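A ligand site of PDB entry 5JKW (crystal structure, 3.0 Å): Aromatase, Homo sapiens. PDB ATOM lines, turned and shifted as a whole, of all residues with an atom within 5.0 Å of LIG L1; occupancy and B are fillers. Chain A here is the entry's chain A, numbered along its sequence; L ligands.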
ATOM      1  N   MET A 107      36.238  13.415  -5.407  1.00  0.00           N
ATOM      2  CA  MET A 107      34.793  13.516  -5.095  1.00  0.00           C
ATOM      3  C   MET A 107      33.936  12.628  -6.004  1.00  0.00           C
ATOM      4  O   MET A 107      32.865  12.184  -5.602  1.00  0.00           O
ATOM      5  CB  MET A 107      34.317  14.975  -5.143  1.00  0.00           C
ATOM      6  CG  MET A 107      35.087  15.892  -4.187  1.00  0.00           C
ATOM      7  SD  MET A 107      34.311  17.432  -3.673  1.00  0.00           S
ATOM      8  CE  MET A 107      33.871  18.115  -5.242  1.00  0.00           C
ATOM      9  N   ARG A 115      35.430  10.411   5.534  1.00  0.00           N
ATOM     10  CA  ARG A 115      36.207  11.529   6.079  1.00  0.00           C
ATOM     11  C   ARG A 115      37.210  10.941   7.090  1.00  0.00           C
ATOM     12  O   ARG A 115      37.502   9.744   7.051  1.00  0.00           O
ATOM     13  CB  ARG A 115      35.265  12.550   6.732  1.00  0.00           C
ATOM     14  CG  ARG A 115      34.041  12.865   5.899  1.00  0.00           C
ATOM     15  CD  ARG A 115      33.426  14.200   6.255  1.00  0.00           C
ATOM     16  NE  ARG A 115      32.219  14.395   5.445  1.00  0.00           N
ATOM     17  CZ  ARG A 115      32.185  14.884   4.209  1.00  0.00           C
ATOM     18  NH1 ARG A 115      33.280  15.286   3.577  1.00  0.00           N
ATOM     19  NH2 ARG A 115      31.008  14.983   3.594  1.00  0.00           N
ATOM     20  N   ILE A 132      25.750  11.010   9.882  1.00  0.00           N
ATOM     21  CA  ILE A 132      26.395  10.896   8.577  1.00  0.00           C
ATOM     22  C   ILE A 132      27.573  11.815   8.326  1.00  0.00           C
ATOM     23  O   ILE A 132      28.433  11.444   7.539  1.00  0.00           O
ATOM     24  CB  ILE A 132      25.413  11.057   7.395  1.00  0.00           C
ATOM     25  CG1 ILE A 132      24.694  12.399   7.422  1.00  0.00           C
ATOM     26  CG2 ILE A 132      24.405   9.922   7.386  1.00  0.00           C
ATOM     27  CD1 ILE A 132      24.060  12.693   6.085  1.00  0.00           C
ATOM     28  N   ILE A 133      27.651  12.968   8.983  1.00  0.00           N
ATOM     29  CA  ILE A 133      28.610  13.997   8.555  1.00  0.00           C
ATOM     30  C   ILE A 133      30.034  13.475   8.698  1.00  0.00           C
ATOM     31  O   ILE A 133      30.795  13.551   7.753  1.00  0.00           O
ATOM     32  CB  ILE A 133      28.466  15.332   9.302  1.00  0.00           C
ATOM     33  CG1 ILE A 133      27.064  15.905   9.098  1.00  0.00           C
ATOM     34  CG2 ILE A 133      29.475  16.343   8.767  1.00  0.00           C
ATOM     35  CD1 ILE A 133      26.700  16.978  10.112  1.00  0.00           C
ATOM     36  N   TRP A 141      27.294   4.404   7.067  1.00  0.00           N
ATOM     37  CA  TRP A 141      27.096   5.634   6.291  1.00  0.00           C
ATOM     38  C   TRP A 141      26.182   5.423   5.097  1.00  0.00           C
ATOM     39  O   TRP A 141      25.265   6.214   4.885  1.00  0.00           O
ATOM     40  CB  TRP A 141      28.443   6.198   5.818  1.00  0.00           C
ATOM     41  CG  TRP A 141      28.311   7.336   4.858  1.00  0.00           C
ATOM     42  CD1 TRP A 141      27.995   8.631   5.152  1.00  0.00           C
ATOM     43  CD2 TRP A 141      28.463   7.268   3.437  1.00  0.00           C
ATOM     44  NE1 TRP A 141      27.952   9.376   3.999  1.00  0.00           N
ATOM     45  CE2 TRP A 141      28.228   8.565   2.938  1.00  0.00           C
ATOM     46  CE3 TRP A 141      28.765   6.239   2.540  1.00  0.00           C
ATOM     47  CZ2 TRP A 141      28.294   8.859   1.574  1.00  0.00           C
ATOM     48  CZ3 TRP A 141      28.840   6.531   1.200  1.00  0.00           C
ATOM     49  CH2 TRP A 141      28.606   7.832   0.722  1.00  0.00           C
ATOM     50  N   ARG A 145      22.633   7.674   4.953  1.00  0.00           N
ATOM     51  CA  ARG A 145      22.554   8.812   4.042  1.00  0.00           C
ATOM     52  C   ARG A 145      21.213   8.948   3.308  1.00  0.00           C
ATOM     53  O   ARG A 145      20.671  10.048   3.245  1.00  0.00           O
ATOM     54  CB  ARG A 145      23.712   8.795   3.036  1.00  0.00           C
ATOM     55  CG  ARG A 145      23.702   9.966   2.067  1.00  0.00           C
ATOM     56  CD  ARG A 145      25.059  10.104   1.400  1.00  0.00           C
ATOM     57  NE  ARG A 145      25.028  10.987   0.230  1.00  0.00           N
ATOM     58  CZ  ARG A 145      25.483  12.243   0.173  1.00  0.00           C
ATOM     59  NH1 ARG A 145      26.010  12.853   1.226  1.00  0.00           N
ATOM     60  NH2 ARG A 145      25.398  12.909  -0.971  1.00  0.00           N
ATOM     61  N   PHE A 148      18.627  11.218   4.812  1.00  0.00           N
ATOM     62  CA  PHE A 148      18.914  12.639   4.652  1.00  0.00           C
ATOM     63  C   PHE A 148      18.561  13.095   3.253  1.00  0.00           C
ATOM     64  O   PHE A 148      17.908  14.124   3.077  1.00  0.00           O
ATOM     65  CB  PHE A 148      20.390  12.945   4.955  1.00  0.00           C
ATOM     66  CG  PHE A 148      20.726  12.915   6.418  1.00  0.00           C
ATOM     67  CD1 PHE A 148      20.956  11.701   7.070  1.00  0.00           C
ATOM     68  CD2 PHE A 148      20.806  14.081   7.150  1.00  0.00           C
ATOM     69  CE1 PHE A 148      21.263  11.669   8.421  1.00  0.00           C
ATOM     70  CE2 PHE A 148      21.104  14.053   8.501  1.00  0.00           C
ATOM     71  CZ  PHE A 148      21.339  12.850   9.134  1.00  0.00           C
ATOM     72  N   LEU A 152      15.799  16.105   2.083  1.00  0.00           N
ATOM     73  CA  LEU A 152      16.368  17.337   1.528  1.00  0.00           C
ATOM     74  C   LEU A 152      16.108  17.555   0.029  1.00  0.00           C
ATOM     75  O   LEU A 152      16.805  18.338  -0.611  1.00  0.00           O
ATOM     76  CB  LEU A 152      17.874  17.362   1.818  1.00  0.00           C
ATOM     77  CG  LEU A 152      18.287  17.338   3.297  1.00  0.00           C
ATOM     78  CD1 LEU A 152      19.789  17.149   3.446  1.00  0.00           C
ATOM     79  CD2 LEU A 152      17.842  18.614   4.001  1.00  0.00           C
ATOM     80  N   PHE A 203      11.765  19.173   9.482  1.00  0.00           N
ATOM     81  CA  PHE A 203      12.322  17.828   9.740  1.00  0.00           C
ATOM     82  C   PHE A 203      11.872  17.124  11.007  1.00  0.00           C
ATOM     83  O   PHE A 203      11.976  15.896  11.086  1.00  0.00           O
ATOM     84  CB  PHE A 203      13.842  17.891   9.742  1.00  0.00           C
ATOM     85  CG  PHE A 203      14.421  18.514   8.510  1.00  0.00           C
ATOM     86  CD1 PHE A 203      14.165  17.975   7.261  1.00  0.00           C
ATOM     87  CD2 PHE A 203      15.219  19.644   8.590  1.00  0.00           C
ATOM     88  CE1 PHE A 203      14.687  18.545   6.121  1.00  0.00           C
ATOM     89  CE2 PHE A 203      15.748  20.231   7.461  1.00  0.00           C
ATOM     90  CZ  PHE A 203      15.476  19.681   6.223  1.00  0.00           C
ATOM     91  N   MET A 303      20.734  16.953  11.576  1.00  0.00           N
ATOM     92  CA  MET A 303      19.849  17.710  10.674  1.00  0.00           C
ATOM     93  C   MET A 303      19.488  19.082  11.253  1.00  0.00           C
ATOM     94  O   MET A 303      19.376  20.069  10.513  1.00  0.00           O
ATOM     95  CB  MET A 303      18.582  16.899  10.365  1.00  0.00           C
ATOM     96  CG  MET A 303      17.683  17.471   9.282  1.00  0.00           C
ATOM     97  SD  MET A 303      18.378  17.317   7.621  1.00  0.00           S
ATOM     98  CE  MET A 303      17.671  15.775   7.048  1.00  0.00           C
ATOM     99  N   ALA A 306      22.719  21.587  11.135  1.00  0.00           N
ATOM    100  CA  ALA A 306      23.359  21.814   9.836  1.00  0.00           C
ATOM    101  C   ALA A 306      23.256  23.254   9.341  1.00  0.00           C
ATOM    102  O   ALA A 306      24.270  23.892   9.070  1.00  0.00           O
ATOM    103  CB  ALA A 306      22.774  20.869   8.786  1.00  0.00           C
ATOM    104  N   ALA A 307      22.029  23.736   9.240  1.00  0.00           N
ATOM    105  CA  ALA A 307      21.777  25.065   8.701  1.00  0.00           C
ATOM    106  C   ALA A 307      22.241  26.187   9.655  1.00  0.00           C
ATOM    107  O   ALA A 307      23.000  27.065   9.242  1.00  0.00           O
ATOM    108  CB  ALA A 307      20.309  25.211   8.310  1.00  0.00           C
ATOM    109  N   THR A 310      25.944  26.537   9.215  1.00  0.00           N
ATOM    110  CA  THR A 310      26.526  26.920   7.939  1.00  0.00           C
ATOM    111  C   THR A 310      25.775  28.002   7.155  1.00  0.00           C
ATOM    112  O   THR A 310      26.399  28.908   6.610  1.00  0.00           O
ATOM    113  CB  THR A 310      26.677  25.674   7.065  1.00  0.00           C
ATOM    114  OG1 THR A 310      25.399  25.016   6.949  1.00  0.00           O
ATOM    115  CG2 THR A 310      27.687  24.718   7.705  1.00  0.00           C
ATOM    116  N   MET A 311      24.455  27.894   7.080  1.00  0.00           N
ATOM    117  CA  MET A 311      23.625  28.893   6.388  1.00  0.00           C
ATOM    118  C   MET A 311      23.736  30.263   7.024  1.00  0.00           C
ATOM    119  O   MET A 311      23.819  31.286   6.341  1.00  0.00           O
ATOM    120  CB  MET A 311      22.146  28.500   6.437  1.00  0.00           C
ATOM    121  CG  MET A 311      21.778  27.279   5.620  1.00  0.00           C
ATOM    122  SD  MET A 311      21.600  27.658   3.885  1.00  0.00           S
ATOM    123  CE  MET A 311      20.129  28.681   3.968  1.00  0.00           C
ATOM    124  N   SER A 314      26.992  31.929   6.225  1.00  0.00           N
ATOM    125  CA  SER A 314      27.077  32.210   4.782  1.00  0.00           C
ATOM    126  C   SER A 314      26.263  33.442   4.432  1.00  0.00           C
ATOM    127  O   SER A 314      26.746  34.331   3.724  1.00  0.00           O
ATOM    128  CB  SER A 314      26.580  31.015   3.963  1.00  0.00           C
ATOM    129  OG  SER A 314      27.354  29.868   4.245  1.00  0.00           O
ATOM    130  N   MET A 364      29.943  32.717  -2.069  1.00  0.00           N
ATOM    131  CA  MET A 364      30.561  31.465  -1.571  1.00  0.00           C
ATOM    132  C   MET A 364      31.923  31.211  -2.187  1.00  0.00           C
ATOM    133  O   MET A 364      32.773  30.584  -1.561  1.00  0.00           O
ATOM    134  CB  MET A 364      29.676  30.259  -1.884  1.00  0.00           C
ATOM    135  CG  MET A 364      28.305  30.273  -1.248  1.00  0.00           C
ATOM    136  SD  MET A 364      27.257  29.024  -2.013  1.00  0.00           S
ATOM    137  CE  MET A 364      27.736  27.658  -0.986  1.00  0.00           C
ATOM    138  N   VAL A 370      32.544  27.127   4.229  1.00  0.00           N
ATOM    139  CA  VAL A 370      33.071  25.758   4.139  1.00  0.00           C
ATOM    140  C   VAL A 370      34.106  25.749   3.034  1.00  0.00           C
ATOM    141  O   VAL A 370      33.824  25.398   1.889  1.00  0.00           O
ATOM    142  CB  VAL A 370      31.953  24.727   3.862  1.00  0.00           C
ATOM    143  CG1 VAL A 370      32.498  23.312   3.976  1.00  0.00           C
ATOM    144  CG2 VAL A 370      30.791  24.919   4.822  1.00  0.00           C
ATOM    145  N   VAL A 373      37.394  20.460   2.765  1.00  0.00           N
ATOM    146  CA  VAL A 373      36.670  19.204   2.843  1.00  0.00           C
ATOM    147  C   VAL A 373      37.609  18.074   3.211  1.00  0.00           C
ATOM    148  O   VAL A 373      38.656  17.920   2.587  1.00  0.00           O
ATOM    149  CB  VAL A 373      36.052  18.830   1.484  1.00  0.00           C
ATOM    150  CG1 VAL A 373      35.363  17.470   1.547  1.00  0.00           C
ATOM    151  CG2 VAL A 373      35.089  19.919   1.027  1.00  0.00           C
ATOM    152  N   ARG A 375      38.437  14.116   3.460  1.00  0.00           N
ATOM    153  CA  ARG A 375      38.130  12.801   2.914  1.00  0.00           C
ATOM    154  C   ARG A 375      39.213  11.788   3.276  1.00  0.00           C
ATOM    155  O   ARG A 375      40.244  12.131   3.827  1.00  0.00           O
ATOM    156  CB  ARG A 375      37.993  12.866   1.400  1.00  0.00           C
ATOM    157  CG  ARG A 375      36.931  13.840   0.903  1.00  0.00           C
ATOM    158  CD  ARG A 375      35.533  13.529   1.410  1.00  0.00           C
ATOM    159  NE  ARG A 375      34.501  13.969   0.484  1.00  0.00           N
ATOM    160  CZ  ARG A 375      34.117  13.311  -0.606  1.00  0.00           C
ATOM    161  NH1 ARG A 375      34.691  12.147  -0.927  1.00  0.00           N
ATOM    162  NH2 ARG A 375      33.154  13.800  -1.386  1.00  0.00           N
ATOM    163  N   ILE A 398      39.173  23.669  -1.169  1.00  0.00           N
ATOM    164  CA  ILE A 398      38.331  24.224  -2.241  1.00  0.00           C
ATOM    165  C   ILE A 398      38.302  25.756  -2.248  1.00  0.00           C
ATOM    166  O   ILE A 398      38.043  26.343  -3.295  1.00  0.00           O
ATOM    167  CB  ILE A 398      36.883  23.662  -2.249  1.00  0.00           C
ATOM    168  CG1 ILE A 398      36.131  23.992  -0.959  1.00  0.00           C
ATOM    169  CG2 ILE A 398      36.899  22.156  -2.470  1.00  0.00           C
ATOM    170  CD1 ILE A 398      34.627  23.929  -1.119  1.00  0.00           C
ATOM    171  N   PRO A 429      31.406  24.527  -4.465  1.00  0.00           N
ATOM    172  CA  PRO A 429      31.148  25.077  -3.139  1.00  0.00           C
ATOM    173  C   PRO A 429      30.459  24.096  -2.188  1.00  0.00           C
ATOM    174  O   PRO A 429      30.609  24.226  -0.976  1.00  0.00           O
ATOM    175  CB  PRO A 429      30.213  26.252  -3.440  1.00  0.00           C
ATOM    176  CG  PRO A 429      29.512  25.868  -4.680  1.00  0.00           C
ATOM    177  CD  PRO A 429      30.547  25.148  -5.491  1.00  0.00           C
ATOM    178  N   PHE A 430      29.681  23.167  -2.742  1.00  0.00           N
ATOM    179  CA  PHE A 430      28.996  22.153  -1.963  1.00  0.00           C
ATOM    180  C   PHE A 430      29.646  20.771  -2.035  1.00  0.00           C
ATOM    181  O   PHE A 430      29.250  19.885  -1.288  1.00  0.00           O
ATOM    182  CB  PHE A 430      27.557  22.008  -2.456  1.00  0.00           C
ATOM    183  CG  PHE A 430      26.712  23.237  -2.261  1.00  0.00           C
ATOM    184  CD1 PHE A 430      26.249  23.956  -3.370  1.00  0.00           C
ATOM    185  CD2 PHE A 430      26.350  23.655  -0.999  1.00  0.00           C
ATOM    186  CE1 PHE A 430      25.462  25.084  -3.208  1.00  0.00           C
ATOM    187  CE2 PHE A 430      25.553  24.784  -0.824  1.00  0.00           C
ATOM    188  CZ  PHE A 430      25.108  25.496  -1.933  1.00  0.00           C
ATOM    189  N   GLY A 431      30.596  20.563  -2.940  1.00  0.00           N
ATOM    190  CA  GLY A 431      31.030  19.207  -3.305  1.00  0.00           C
ATOM    191  C   GLY A 431      29.967  18.508  -4.179  1.00  0.00           C
ATOM    192  O   GLY A 431      28.840  18.995  -4.304  1.00  0.00           O
ATOM    193  N   PHE A 432      30.333  17.369  -4.772  1.00  0.00           N
ATOM    194  CA  PHE A 432      29.399  16.541  -5.569  1.00  0.00           C
ATOM    195  C   PHE A 432      29.734  15.059  -5.419  1.00  0.00           C
ATOM    196  O   PHE A 432      30.679  14.680  -4.715  1.00  0.00           O
ATOM    197  CB  PHE A 432      29.430  16.954  -7.058  1.00  0.00           C
ATOM    198  CG  PHE A 432      30.645  16.454  -7.780  1.00  0.00           C
ATOM    199  CD1 PHE A 432      30.607  15.284  -8.530  1.00  0.00           C
ATOM    200  CD2 PHE A 432      31.845  17.131  -7.684  1.00  0.00           C
ATOM    201  CE1 PHE A 432      31.747  14.819  -9.174  1.00  0.00           C
ATOM    202  CE2 PHE A 432      32.989  16.676  -8.310  1.00  0.00           C
ATOM    203  CZ  PHE A 432      32.939  15.507  -9.047  1.00  0.00           C
ATOM    204  N   ARG A 435      29.157  11.475  -1.946  1.00  0.00           N
ATOM    205  CA  ARG A 435      29.251  12.076  -0.594  1.00  0.00           C
ATOM    206  C   ARG A 435      29.292  13.622  -0.613  1.00  0.00           C
ATOM    207  O   ARG A 435      29.788  14.249   0.317  1.00  0.00           O
ATOM    208  CB  ARG A 435      30.493  11.523   0.131  1.00  0.00           C
ATOM    209  CG  ARG A 435      30.556  11.893   1.595  1.00  0.00           C
ATOM    210  CD  ARG A 435      31.116  10.799   2.486  1.00  0.00           C
ATOM    211  NE  ARG A 435      30.770  11.081   3.876  1.00  0.00           N
ATOM    212  CZ  ARG A 435      30.990  10.253   4.888  1.00  0.00           C
ATOM    213  NH1 ARG A 435      31.572   9.069   4.709  1.00  0.00           N
ATOM    214  NH2 ARG A 435      30.620  10.622   6.110  1.00  0.00           N
ATOM    215  N   GLY A 436      28.747  14.221  -1.667  1.00  0.00           N
ATOM    216  CA  GLY A 436      28.616  15.681  -1.727  1.00  0.00           C
ATOM    217  C   GLY A 436      27.582  16.147  -0.725  1.00  0.00           C
ATOM    218  O   GLY A 436      26.898  15.311  -0.115  1.00  0.00           O
ATOM    219  N   CYS A 437      27.459  17.457  -0.552  1.00  0.00           N
ATOM    220  CA  CYS A 437      26.549  18.018   0.438  1.00  0.00           C
ATOM    221  C   CYS A 437      25.142  17.484   0.202  1.00  0.00           C
ATOM    222  O   CYS A 437      24.625  17.607  -0.887  1.00  0.00           O
ATOM    223  CB  CYS A 437      26.541  19.543   0.360  1.00  0.00           C
ATOM    224  SG  CYS A 437      25.378  20.347   1.491  1.00  0.00           S
ATOM    225  N   ALA A 438      24.539  16.889   1.219  1.00  0.00           N
ATOM    226  CA  ALA A 438      23.174  16.394   1.117  1.00  0.00           C
ATOM    227  C   ALA A 438      22.189  17.541   1.022  1.00  0.00           C
ATOM    228  O   ALA A 438      21.084  17.369   0.524  1.00  0.00           O
ATOM    229  CB  ALA A 438      22.836  15.504   2.296  1.00  0.00           C
ATOM    230  N   GLY A 439      22.569  18.711   1.534  1.00  0.00           N
ATOM    231  CA  GLY A 439      21.725  19.889   1.438  1.00  0.00           C
ATOM    232  C   GLY A 439      21.919  20.765   0.227  1.00  0.00           C
ATOM    233  O   GLY A 439      21.263  21.794   0.123  1.00  0.00           O
ATOM    234  N   ALA A 443      19.717  24.054   0.045  1.00  0.00           N
ATOM    235  CA  ALA A 443      20.466  25.182   0.589  1.00  0.00           C
ATOM    236  C   ALA A 443      20.295  26.388  -0.297  1.00  0.00           C
ATOM    237  O   ALA A 443      19.973  27.466   0.180  1.00  0.00           O
ATOM    238  CB  ALA A 443      21.950  24.837   0.707  1.00  0.00           C
ATOM    239  N   MET A 446      16.869  27.719   0.124  1.00  0.00           N
ATOM    240  CA  MET A 446      16.755  28.415   1.413  1.00  0.00           C
ATOM    241  C   MET A 446      17.399  29.798   1.393  1.00  0.00           C
ATOM    242  O   MET A 446      16.787  30.767   1.855  1.00  0.00           O
ATOM    243  CB  MET A 446      17.361  27.568   2.536  1.00  0.00           C
ATOM    244  CG  MET A 446      16.573  26.311   2.890  1.00  0.00           C
ATOM    245  SD  MET A 446      16.885  25.665   4.546  1.00  0.00           S
ATOM    246  CE  MET A 446      18.621  25.262   4.492  1.00  0.00           C
ATOM    247  N   MET A 447      18.616  29.892   0.855  1.00  0.00           N
ATOM    248  CA  MET A 447      19.331  31.179   0.796  1.00  0.00           C
ATOM    249  C   MET A 447      18.601  32.226  -0.043  1.00  0.00           C
ATOM    250  O   MET A 447      18.589  33.401   0.334  1.00  0.00           O
ATOM    251  CB  MET A 447      20.774  31.004   0.304  1.00  0.00           C
ATOM    252  CG  MET A 447      21.663  30.380   1.361  1.00  0.00           C
ATOM    253  SD  MET A 447      23.425  30.343   1.016  1.00  0.00           S
ATOM    254  CE  MET A 447      23.543  28.866   0.016  1.00  0.00           C
HETATM  255  C1  LIG L   1      28.426  18.088   3.605  1.00  0.00           C
HETATM  256  C2  LIG L   1      28.760  22.678   2.153  1.00  0.00           C
HETATM  257  C3  LIG L   1      24.320  23.514   3.877  1.00  0.00           C
HETATM  258  C4  LIG L   1      23.950  18.929   5.167  1.00  0.00           C
HETATM  259  C5  LIG L   1      28.874  19.255   3.032  1.00  0.00           C
HETATM  260  C6  LIG L   1      30.112  19.390   2.380  1.00  0.00           C
HETATM  261  C7  LIG L   1      30.214  20.676   1.973  1.00  0.00           C
HETATM  262  C8  LIG L   1      29.032  21.340   2.359  1.00  0.00           C
HETATM  263  C9  LIG L   1      31.405  21.230   1.228  1.00  0.00           C
HETATM  264  C10 LIG L   1      31.152  18.327   2.150  1.00  0.00           C
HETATM  265  C11 LIG L   1      30.694  17.473   0.958  1.00  0.00           C
HETATM  266  C12 LIG L   1      31.845  16.660   0.395  1.00  0.00           C
HETATM  267  O1  LIG L   1      32.635  16.058   1.149  1.00  0.00           O
HETATM  268  O2  LIG L   1      31.997  16.557  -0.838  1.00  0.00           O
HETATM  269  C13 LIG L   1      27.586  23.333   2.531  1.00  0.00           C
HETATM  270  C14 LIG L   1      27.347  24.726   2.331  1.00  0.00           C
HETATM  271  C15 LIG L   1      26.080  24.990   2.815  1.00  0.00           C
HETATM  272  C16 LIG L   1      25.587  23.678   3.321  1.00  0.00           C
HETATM  273  C17 LIG L   1      28.356  25.646   1.686  1.00  0.00           C
HETATM  274  C18 LIG L   1      25.254  26.230   2.892  1.00  0.00           C
HETATM  275  C19 LIG L   1      25.588  27.449   2.490  1.00  0.00           C
HETATM  276  C20 LIG L   1      23.796  22.337   4.353  1.00  0.00           C
HETATM  277  C21 LIG L   1      22.494  22.164   4.875  1.00  0.00           C
HETATM  278  C22 LIG L   1      22.372  20.824   5.248  1.00  0.00           C
HETATM  279  C23 LIG L   1      23.629  20.222   4.939  1.00  0.00           C
HETATM  280  C24 LIG L   1      21.444  23.245   4.977  1.00  0.00           C
HETATM  281  C25 LIG L   1      21.221  20.089   5.870  1.00  0.00           C
HETATM  282  C26 LIG L   1      20.039  20.613   6.223  1.00  0.00           C
HETATM  283  C27 LIG L   1      25.176  18.382   4.843  1.00  0.00           C
HETATM  284  C28 LIG L   1      25.452  16.984   5.169  1.00  0.00           C
HETATM  285  C29 LIG L   1      26.676  16.724   4.739  1.00  0.00           C
HETATM  286  C30 LIG L   1      27.167  17.999   4.161  1.00  0.00           C
HETATM  287  C31 LIG L   1      24.518  16.013   5.842  1.00  0.00           C
HETATM  288  C32 LIG L   1      27.413  15.415   4.878  1.00  0.00           C
HETATM  289  C33 LIG L   1      27.240  14.491   3.682  1.00  0.00           C
HETATM  290  C34 LIG L   1      27.978  13.195   3.932  1.00  0.00           C
HETATM  291  O3  LIG L   1      27.489  12.135   3.494  1.00  0.00           O
HETATM  292  O4  LIG L   1      29.064  13.167   4.558  1.00  0.00           O
HETATM  293  N1  LIG L   1      28.209  20.457   3.003  1.00  0.00           N
HETATM  294  N2  LIG L   1      26.528  22.771   3.086  1.00  0.00           N
HETATM  295  N3  LIG L   1      24.458  21.157   4.393  1.00  0.00           N
HETATM  296  N4  LIG L   1      26.223  18.964   4.218  1.00  0.00           N
HETATM  297 FE1  LIG L   1      26.365  20.773   3.659  1.00  0.00          FE
HETATM  298  C1  LG2 L   2      28.100  19.998   7.817  1.00  0.00           C
HETATM  299  C2  LG2 L   2      26.868  20.612   8.471  1.00  0.00           C
HETATM  300  C3  LG2 L   2      27.285  21.392   9.681  1.00  0.00           C
HETATM  301  O1  LG2 L   2      26.545  21.427  10.650  1.00  0.00           O
HETATM  302  C4  LG2 L   2      28.589  22.082   9.712  1.00  0.00           C
HETATM  303  C5  LG2 L   2      29.468  21.933   8.701  1.00  0.00           C
HETATM  304  C6  LG2 L   2      30.725  22.776   8.719  1.00  0.00           C
HETATM  305  C7  LG2 L   2      31.956  21.902   8.559  1.00  0.00           C
HETATM  306  C8  LG2 L   2      31.824  20.998   7.342  1.00  0.00           C
HETATM  307  C9  LG2 L   2      30.563  20.129   7.449  1.00  0.00           C
HETATM  308  C10 LG2 L   2      29.262  20.957   7.557  1.00  0.00           C
HETATM  309  C11 LG2 L   2      30.536  19.039   6.360  1.00  0.00           C
HETATM  310  C12 LG2 L   2      31.819  18.224   6.296  1.00  0.00           C
HETATM  311  C13 LG2 L   2      33.027  19.115   6.115  1.00  0.00           C
HETATM  312  C14 LG2 L   2      33.059  20.113   7.259  1.00  0.00           C
HETATM  313  C15 LG2 L   2      34.432  20.748   7.143  1.00  0.00           C
HETATM  314  C16 LG2 L   2      35.328  19.574   6.724  1.00  0.00           C
HETATM  315  C17 LG2 L   2      34.361  18.431   6.378  1.00  0.00           C
HETATM  316  O2  LG2 L   2      34.817  17.588   5.322  1.00  0.00           O
HETATM  317  C18 LG2 L   2      33.020  19.768   4.725  1.00  0.00           C
HETATM  318  C19 LG2 L   2      28.952  21.751   6.297  1.00  0.00           C
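NH1 of Arg 115 lies within salt-bridge range of O1 of LIG L1 (2.6 Å). NE of Arg 375 is in salt-bridge range of O1 of LIG L1 (2.9 Å). The guanidinium group of Arg 435 is in salt-bridge range of an oxygen (O4) of LIG L1, at 2.8 Å. O2 of LG2 L2 lies within hydrogen-bond range of NH1 of Arg 115. FE1 of LIG L1 is bound by SG of Cys 437 (2.4 Å). An oxygen (O3) of LIG L1 is in hydrogen-bond range of the indole nitrogen of Trp 141. O3 of LIG L1 is in salt-bridge range of NH1 of Arg 145, at 2.8 Å.
The backbone NH of Gly 439 sits close to the side-chain sulfur of Cys 437. The side-chain hydroxyl (OG) of Ser 314 is in hydrogen-bond range of the backbone carbonyl oxygen (O) of Thr 310 (2.7 Å). The side-chain hydroxyl (OG1) of Thr 310 is in hydrogen-bond range of the backbone carbonyl oxygen (O) of Ala 306, 2.7 Å away. NH2 of Arg 435 lies within hydrogen-bond range of O of Ile 132, at 2.7 Å. The backbone carbonyl oxygen (O) of Ile 133 is in hydrogen-bond range of the guanidinium group (NE) of Arg 115 (2.8 Å). The backbone NH of Cys 437 is in hydrogen-bond range of the backbone carbonyl oxygen of Phe 430. NH2 of Arg 435 is in hydrogen-bond range of O of Ile 133 (3.4 Å). The backbone carbonyl oxygen (O) of Gly 436 lies within hydrogen-bond range of the guanidinium group (NH1) of Arg 145 (2.9 Å).
The side-chain sulfur (SD) of Met 107 sits close to an oxygen (O2) of LIG L1, at 3.8 Å. Merely in contact with LIG L1: Ile 132, Ile 133, Leu 152, Met 303, Ala 306, Thr 310, Ser 314, Met 364, Val 370, Val 373, Pro 429, Phe 430, Gly 431, Gly 436, Ala 438, Gly 439, Met 446 and Met 447. Hydrophobic or aromatic side chains that line LIG L1: Met 107, Ile 132, Trp 141, Leu 152, Met 303, Ala 306, Met 364, Val 370, Val 373, Phe 430, Ala 438, Met 446 and Met 447. Within 4 Å of LIG L1: Met 107, Arg 115, Ile 132, Ile 133, Trp 141, Arg 145, Leu 152, Met 303, Ala 306, Thr 310, Ser 314, Met 364, Val 370, Val 373, Arg 375, Pro 429, Phe 430, Gly 431, Arg 435, Gly 436, Cys 437, Ala 438, Gly 439, Met 446 and Met 447. The nearest printed residue that does not touch LIG L1 is Ala 307 (4.03 Å).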
